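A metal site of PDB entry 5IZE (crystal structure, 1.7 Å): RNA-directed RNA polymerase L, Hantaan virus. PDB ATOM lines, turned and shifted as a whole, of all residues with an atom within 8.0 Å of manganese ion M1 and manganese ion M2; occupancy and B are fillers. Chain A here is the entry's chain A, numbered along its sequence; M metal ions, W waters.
Manganese ion M2 is bound by water W4 (2.1 Å), water W3 (2.2 Å), the side-chain carboxylate of Asp 98 (2.2 Å), the side-chain carboxylate of Glu 55 (2.3 Å), water W5 (2.3 Å) and water W2 (2.4 Å).
The nearest printed residue that does not touch manganese ion M1 is Lys 125 (4.3 Å).
OE1 of Glu 55 sits at hydrogen-bond distance from OG1 of Thr 96 (3.3 Å). The backbone carbonyl oxygen of Glu 111 lies within hydrogen-bond range of the backbone NH of Val 160 (2.9 Å). OD1 of Asp 38 lies within hydrogen-bond range of ND1 of His 37. O of Asp 98 lies within hydrogen-bond range of NZ of Lys 45. The side-chain amino group of Lys 125 lies close to the side-chain carboxylate of Glu 111, at 3.3 Å.
Manganese ion M1 is bound by OD2 of Asp 98 (2.2 Å), water W4 (2.2 Å), O of Val 112 (2.2 Å), OE2 of Glu 111 (2.2 Å), water W1 (2.2 Å) and NE2 of His 37 (2.3 Å). Manganese ion M1 has six donor atoms within binding distance.
Of the 22 residues printed, 2 come within 4 Å of manganese ion M2. Along chain A the residues within 4 Å of manganese ion M2 span positions 55 to 98.
Water W5 lies within hydrogen-bond range of O of Thr 96 (2.8 Å), OE1 of Glu 111 (2.8 Å) and N of Asp 98 (3.5 Å).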
ATOM      1  N   HIS A  37     -22.360   3.411  -5.573  1.00  0.00           N
ATOM      2  CA  HIS A  37     -23.337   3.656  -4.507  1.00  0.00           C
ATOM      3  C   HIS A  37     -24.158   4.904  -4.806  1.00  0.00           C
ATOM      4  O   HIS A  37     -25.395   4.897  -4.779  1.00  0.00           O
ATOM      5  CB  HIS A  37     -22.624   3.843  -3.189  1.00  0.00           C
ATOM      6  CG  HIS A  37     -23.538   4.229  -2.068  1.00  0.00           C
ATOM      7  ND1 HIS A  37     -23.989   5.522  -1.886  1.00  0.00           N
ATOM      8  CD2 HIS A  37     -24.082   3.500  -1.071  1.00  0.00           C
ATOM      9  CE1 HIS A  37     -24.748   5.572  -0.811  1.00  0.00           C
ATOM     10  NE2 HIS A  37     -24.822   4.358  -0.300  1.00  0.00           N
ATOM     11  N   ASP A  38     -23.446   5.980  -5.140  1.00  0.00           N
ATOM     12  CA  ASP A  38     -24.099   7.265  -5.359  1.00  0.00           C
ATOM     13  C   ASP A  38     -25.012   7.282  -6.581  1.00  0.00           C
ATOM     14  O   ASP A  38     -26.090   7.909  -6.545  1.00  0.00           O
ATOM     15  CB  ASP A  38     -23.068   8.380  -5.370  1.00  0.00           C
ATOM     16  CG  ASP A  38     -22.474   8.614  -3.983  1.00  0.00           C
ATOM     17  OD1 ASP A  38     -22.967   8.038  -2.962  1.00  0.00           O
ATOM     18  OD2 ASP A  38     -21.501   9.353  -3.907  1.00  0.00           O
ATOM     19  N   ASP A  41     -28.107   5.282  -5.553  1.00  0.00           N
ATOM     20  CA  ASP A  41     -28.829   6.169  -4.644  1.00  0.00           C
ATOM     21  C   ASP A  41     -29.590   7.278  -5.418  1.00  0.00           C
ATOM     22  O   ASP A  41     -30.762   7.538  -5.141  1.00  0.00           O
ATOM     23  CB  ASP A  41     -27.852   6.777  -3.647  1.00  0.00           C
ATOM     24  CG  ASP A  41     -28.544   7.553  -2.558  1.00  0.00           C
ATOM     25  OD1 ASP A  41     -29.423   7.007  -1.902  1.00  0.00           O
ATOM     26  OD2 ASP A  41     -28.224   8.739  -2.375  1.00  0.00           O
ATOM     27  N   LYS A  45     -33.583   8.203  -5.691  1.00  0.00           N
ATOM     28  CA  LYS A  45     -33.998   9.593  -5.437  1.00  0.00           C
ATOM     29  C   LYS A  45     -34.797  10.187  -6.582  1.00  0.00           C
ATOM     30  O   LYS A  45     -35.721  10.975  -6.349  1.00  0.00           O
ATOM     31  CB  LYS A  45     -32.810  10.457  -5.096  1.00  0.00           C
ATOM     32  CG  LYS A  45     -32.282  10.203  -3.714  1.00  0.00           C
ATOM     33  CD  LYS A  45     -31.109  11.100  -3.355  1.00  0.00           C
ATOM     34  CE  LYS A  45     -30.851  11.128  -1.851  1.00  0.00           C
ATOM     35  NZ  LYS A  45     -30.540   9.797  -1.278  1.00  0.00           N
ATOM     36  N   SER A  54     -30.410  15.141  -0.772  1.00  0.00           N
ATOM     37  CA  SER A  54     -29.479  14.436   0.081  1.00  0.00           C
ATOM     38  C   SER A  54     -30.187  13.604   1.117  1.00  0.00           C
ATOM     39  O   SER A  54     -31.385  13.704   1.291  1.00  0.00           O
ATOM     40  CB  SER A  54     -28.475  15.406   0.729  1.00  0.00           C
ATOM     41  OG  SER A  54     -28.947  15.889   1.962  1.00  0.00           O
ATOM     42  N   GLU A  55     -29.428  12.724   1.761  1.00  0.00           N
ATOM     43  CA  GLU A  55     -29.903  11.975   2.911  1.00  0.00           C
ATOM     44  C   GLU A  55     -30.295  12.912   4.066  1.00  0.00           C
ATOM     45  O   GLU A  55     -29.742  13.997   4.212  1.00  0.00           O
ATOM     46  CB  GLU A  55     -28.858  10.959   3.357  1.00  0.00           C
ATOM     47  CG  GLU A  55     -27.545  11.554   3.816  1.00  0.00           C
ATOM     48  CD  GLU A  55     -26.468  10.504   3.906  1.00  0.00           C
ATOM     49  OE1 GLU A  55     -25.374  10.814   4.430  1.00  0.00           O
ATOM     50  OE2 GLU A  55     -26.702   9.352   3.460  1.00  0.00           O
ATOM     51  N   GLU A  56     -31.255  12.487   4.859  1.00  0.00           N
ATOM     52  CA  GLU A  56     -31.875  13.329   5.861  1.00  0.00           C
ATOM     53  C   GLU A  56     -31.779  12.640   7.200  1.00  0.00           C
ATOM     54  O   GLU A  56     -31.843  11.406   7.271  1.00  0.00           O
ATOM     55  CB  GLU A  56     -33.343  13.516   5.454  1.00  0.00           C
ATOM     56  CG  GLU A  56     -34.075  14.594   6.208  1.00  0.00           C
ATOM     57  CD  GLU A  56     -33.503  15.954   5.917  1.00  0.00           C
ATOM     58  OE1 GLU A  56     -33.875  16.548   4.895  1.00  0.00           O
ATOM     59  OE2 GLU A  56     -32.646  16.408   6.706  1.00  0.00           O
ATOM     60  N   THR A  96     -28.553   9.220   9.296  1.00  0.00           N
ATOM     61  CA  THR A  96     -29.038   9.649   7.981  1.00  0.00           C
ATOM     62  C   THR A  96     -29.091   8.470   6.995  1.00  0.00           C
ATOM     63  O   THR A  96     -28.191   8.300   6.154  1.00  0.00           O
ATOM     64  CB  THR A  96     -28.155  10.756   7.391  1.00  0.00           C
ATOM     65  OG1 THR A  96     -26.793  10.312   7.348  1.00  0.00           O
ATOM     66  CG2 THR A  96     -28.222  12.041   8.227  1.00  0.00           C
ATOM     67  N   PRO A  97     -30.149   7.661   7.069  1.00  0.00           N
ATOM     68  CA  PRO A  97     -30.324   6.650   6.020  1.00  0.00           C
ATOM     69  C   PRO A  97     -30.444   7.323   4.647  1.00  0.00           C
ATOM     70  O   PRO A  97     -30.874   8.477   4.545  1.00  0.00           O
ATOM     71  CB  PRO A  97     -31.628   5.934   6.399  1.00  0.00           C
ATOM     72  CG  PRO A  97     -31.977   6.395   7.765  1.00  0.00           C
ATOM     73  CD  PRO A  97     -31.314   7.732   7.978  1.00  0.00           C
ATOM     74  N   ASP A  98     -30.060   6.608   3.591  1.00  0.00           N
ATOM     75  CA  ASP A  98     -29.970   7.217   2.273  1.00  0.00           C
ATOM     76  C   ASP A  98     -31.251   7.840   1.767  1.00  0.00           C
ATOM     77  O   ASP A  98     -31.227   8.991   1.267  1.00  0.00           O
ATOM     78  CB  ASP A  98     -29.468   6.180   1.249  1.00  0.00           C
ATOM     79  CG  ASP A  98     -28.006   5.862   1.405  1.00  0.00           C
ATOM     80  OD1 ASP A  98     -27.241   6.804   1.618  1.00  0.00           O
ATOM     81  OD2 ASP A  98     -27.619   4.669   1.258  1.00  0.00           O
ATOM     82  N   ASN A  99     -32.363   7.123   1.942  1.00  0.00           N
ATOM     83  CA  ASN A  99     -33.635   7.485   1.301  1.00  0.00           C
ATOM     84  C   ASN A  99     -34.794   7.263   2.237  1.00  0.00           C
ATOM     85  O   ASN A  99     -34.801   6.310   3.009  1.00  0.00           O
ATOM     86  CB  ASN A  99     -33.886   6.624   0.052  1.00  0.00           C
ATOM     87  CG  ASN A  99     -32.809   6.824  -0.973  1.00  0.00           C
ATOM     88  OD1 ASN A  99     -32.765   7.852  -1.630  1.00  0.00           O
ATOM     89  ND2 ASN A  99     -31.901   5.868  -1.068  1.00  0.00           N
ATOM     90  N   VAL A 110     -34.966   3.418   2.814  1.00  0.00           N
ATOM     91  CA  VAL A 110     -34.161   2.551   1.931  1.00  0.00           C
ATOM     92  C   VAL A 110     -32.699   2.993   2.011  1.00  0.00           C
ATOM     93  O   VAL A 110     -32.362   4.143   1.681  1.00  0.00           O
ATOM     94  CB  VAL A 110     -34.642   2.598   0.497  1.00  0.00           C
ATOM     95  CG1 VAL A 110     -33.781   1.691  -0.360  1.00  0.00           C
ATOM     96  CG2 VAL A 110     -36.111   2.193   0.413  1.00  0.00           C
ATOM     97  N   GLU A 111     -31.861   2.073   2.478  1.00  0.00           N
ATOM     98  CA  GLU A 111     -30.414   2.273   2.565  1.00  0.00           C
ATOM     99  C   GLU A 111     -29.755   1.484   1.454  1.00  0.00           C
ATOM    100  O   GLU A 111     -30.031   0.322   1.281  1.00  0.00           O
ATOM    101  CB  GLU A 111     -29.933   1.801   3.933  1.00  0.00           C
ATOM    102  CG  GLU A 111     -28.424   1.850   4.143  1.00  0.00           C
ATOM    103  CD  GLU A 111     -27.820   3.238   4.065  1.00  0.00           C
ATOM    104  OE1 GLU A 111     -28.514   4.249   4.376  1.00  0.00           O
ATOM    105  OE2 GLU A 111     -26.617   3.294   3.702  1.00  0.00           O
ATOM    106  N   VAL A 112     -28.864   2.149   0.724  1.00  0.00           N
ATOM    107  CA  VAL A 112     -28.066   1.543  -0.328  1.00  0.00           C
ATOM    108  C   VAL A 112     -26.705   1.132   0.249  1.00  0.00           C
ATOM    109  O   VAL A 112     -26.083   1.881   0.945  1.00  0.00           O
ATOM    110  CB  VAL A 112     -27.842   2.511  -1.492  1.00  0.00           C
ATOM    111  CG1 VAL A 112     -27.033   1.844  -2.623  1.00  0.00           C
ATOM    112  CG2 VAL A 112     -29.163   2.974  -2.068  1.00  0.00           C
ATOM    113  N   THR A 113     -26.281  -0.093  -0.056  1.00  0.00           N
ATOM    114  CA  THR A 113     -24.928  -0.518   0.213  1.00  0.00           C
ATOM    115  C   THR A 113     -24.295  -1.170  -1.035  1.00  0.00           C
ATOM    116  O   THR A 113     -24.955  -1.897  -1.777  1.00  0.00           O
ATOM    117  CB  THR A 113     -24.872  -1.461   1.432  1.00  0.00           C
ATOM    118  OG1 THR A 113     -23.501  -1.709   1.766  1.00  0.00           O
ATOM    119  CG2 THR A 113     -25.597  -2.760   1.169  1.00  0.00           C
ATOM    120  N   VAL A 114     -23.017  -0.871  -1.274  1.00  0.00           N
ATOM    121  CA  VAL A 114     -22.261  -1.524  -2.340  1.00  0.00           C
ATOM    122  C   VAL A 114     -21.217  -2.390  -1.616  1.00  0.00           C
ATOM    123  O   VAL A 114     -20.423  -1.893  -0.842  1.00  0.00           O
ATOM    124  CB  VAL A 114     -21.590  -0.509  -3.274  1.00  0.00           C
ATOM    125  CG1 VAL A 114     -20.759  -1.215  -4.340  1.00  0.00           C
ATOM    126  CG2 VAL A 114     -22.659   0.307  -3.969  1.00  0.00           C
ATOM    127  N   GLU A 124     -25.006  -5.681   8.162  1.00  0.00           N
ATOM    128  CA  GLU A 124     -24.382  -4.456   8.702  1.00  0.00           C
ATOM    129  C   GLU A 124     -25.368  -3.274   8.792  1.00  0.00           C
ATOM    130  O   GLU A 124     -25.416  -2.538   9.801  1.00  0.00           O
ATOM    131  CB  GLU A 124     -23.203  -4.042   7.830  1.00  0.00           C
ATOM    132  CG  GLU A 124     -22.432  -2.821   8.332  1.00  0.00           C
ATOM    133  CD  GLU A 124     -21.991  -1.859   7.234  1.00  0.00           C
ATOM    134  OE1 GLU A 124     -21.317  -2.314   6.277  1.00  0.00           O
ATOM    135  OE2 GLU A 124     -22.307  -0.652   7.342  1.00  0.00           O
ATOM    136  N   LYS A 125     -26.111  -3.076   7.702  1.00  0.00           N
ATOM    137  CA  LYS A 125     -27.082  -1.967   7.628  1.00  0.00           C
ATOM    138  C   LYS A 125     -28.261  -2.177   8.573  1.00  0.00           C
ATOM    139  O   LYS A 125     -28.691  -1.236   9.252  1.00  0.00           O
ATOM    140  CB  LYS A 125     -27.552  -1.706   6.190  1.00  0.00           C
ATOM    141  CG  LYS A 125     -26.473  -1.141   5.274  1.00  0.00           C
ATOM    142  CD  LYS A 125     -25.719   0.047   5.827  1.00  0.00           C
ATOM    143  CE  LYS A 125     -24.825   0.633   4.758  1.00  0.00           C
ATOM    144  NZ  LYS A 125     -24.084   1.816   5.263  1.00  0.00           N
ATOM    145  N   LYS A 128     -27.269  -1.390  12.091  1.00  0.00           N
ATOM    146  CA  LYS A 128     -27.187   0.038  12.275  1.00  0.00           C
ATOM    147  C   LYS A 128     -28.559   0.672  12.561  1.00  0.00           C
ATOM    148  O   LYS A 128     -28.676   1.501  13.437  1.00  0.00           O
ATOM    149  CB  LYS A 128     -26.550   0.639  11.032  1.00  0.00           C
ATOM    150  CG  LYS A 128     -26.198   2.101  11.093  1.00  0.00           C
ATOM    151  CD  LYS A 128     -25.202   2.440   9.998  1.00  0.00           C
ATOM    152  CE  LYS A 128     -24.770   3.892  10.072  1.00  0.00           C
ATOM    153  NZ  LYS A 128     -23.666   4.192   9.128  1.00  0.00           N
ATOM    154  N   TYR A 129     -29.574   0.265  11.809  1.00  0.00           N
ATOM    155  CA  TYR A 129     -30.854   1.011  11.764  1.00  0.00           C
ATOM    156  C   TYR A 129     -32.067   0.331  12.302  1.00  0.00           C
ATOM    157  O   TYR A 129     -33.018   0.979  12.768  1.00  0.00           O
ATOM    158  CB  TYR A 129     -31.179   1.403  10.329  1.00  0.00           C
ATOM    159  CG  TYR A 129     -30.249   2.398   9.756  1.00  0.00           C
ATOM    160  CD1 TYR A 129     -30.243   3.713  10.220  1.00  0.00           C
ATOM    161  CD2 TYR A 129     -29.353   2.036   8.754  1.00  0.00           C
ATOM    162  CE1 TYR A 129     -29.373   4.650   9.686  1.00  0.00           C
ATOM    163  CE2 TYR A 129     -28.491   2.973   8.214  1.00  0.00           C
ATOM    164  CZ  TYR A 129     -28.515   4.285   8.682  1.00  0.00           C
ATOM    165  OH  TYR A 129     -27.684   5.222   8.164  1.00  0.00           O
ATOM    166  N   VAL A 159     -33.075  -2.527   2.604  1.00  0.00           N
ATOM    167  CA  VAL A 159     -31.688  -2.378   2.147  1.00  0.00           C
ATOM    168  C   VAL A 159     -31.655  -2.816   0.678  1.00  0.00           C
ATOM    169  O   VAL A 159     -32.186  -3.879   0.332  1.00  0.00           O
ATOM    170  CB  VAL A 159     -30.676  -3.225   2.941  1.00  0.00           C
ATOM    171  CG1 VAL A 159     -29.235  -2.894   2.503  1.00  0.00           C
ATOM    172  CG2 VAL A 159     -30.794  -2.989   4.426  1.00  0.00           C
ATOM    173  N   VAL A 160     -31.055  -1.981  -0.161  1.00  0.00           N
ATOM    174  CA  VAL A 160     -30.726  -2.303  -1.529  1.00  0.00           C
ATOM    175  C   VAL A 160     -29.221  -2.575  -1.533  1.00  0.00           C
ATOM    176  O   VAL A 160     -28.436  -1.662  -1.299  1.00  0.00           O
ATOM    177  CB  VAL A 160     -31.109  -1.162  -2.494  1.00  0.00           C
ATOM    178  CG1 VAL A 160     -30.588  -1.391  -3.886  1.00  0.00           C
ATOM    179  CG2 VAL A 160     -32.635  -1.044  -2.535  1.00  0.00           C
HETATM  180 MN    MN M   1     -25.675   3.864   1.798  1.00  0.00          MN
HETATM  181 MN    MN M   2     -25.642   7.401   2.991  1.00  0.00          MN
HETATM  182  O   HOH W   1     -23.724   3.044   2.504  1.00  0.00           O
HETATM  183  O   HOH W   2     -24.514   8.558   1.266  1.00  0.00           O
HETATM  184  O   HOH W   3     -24.256   8.348   4.341  1.00  0.00           O
HETATM  185  O   HOH W   4     -24.605   5.545   2.683  1.00  0.00           O
HETATM  186  O   HOH W   5     -26.764   6.417   4.718  1.00  0.00           O
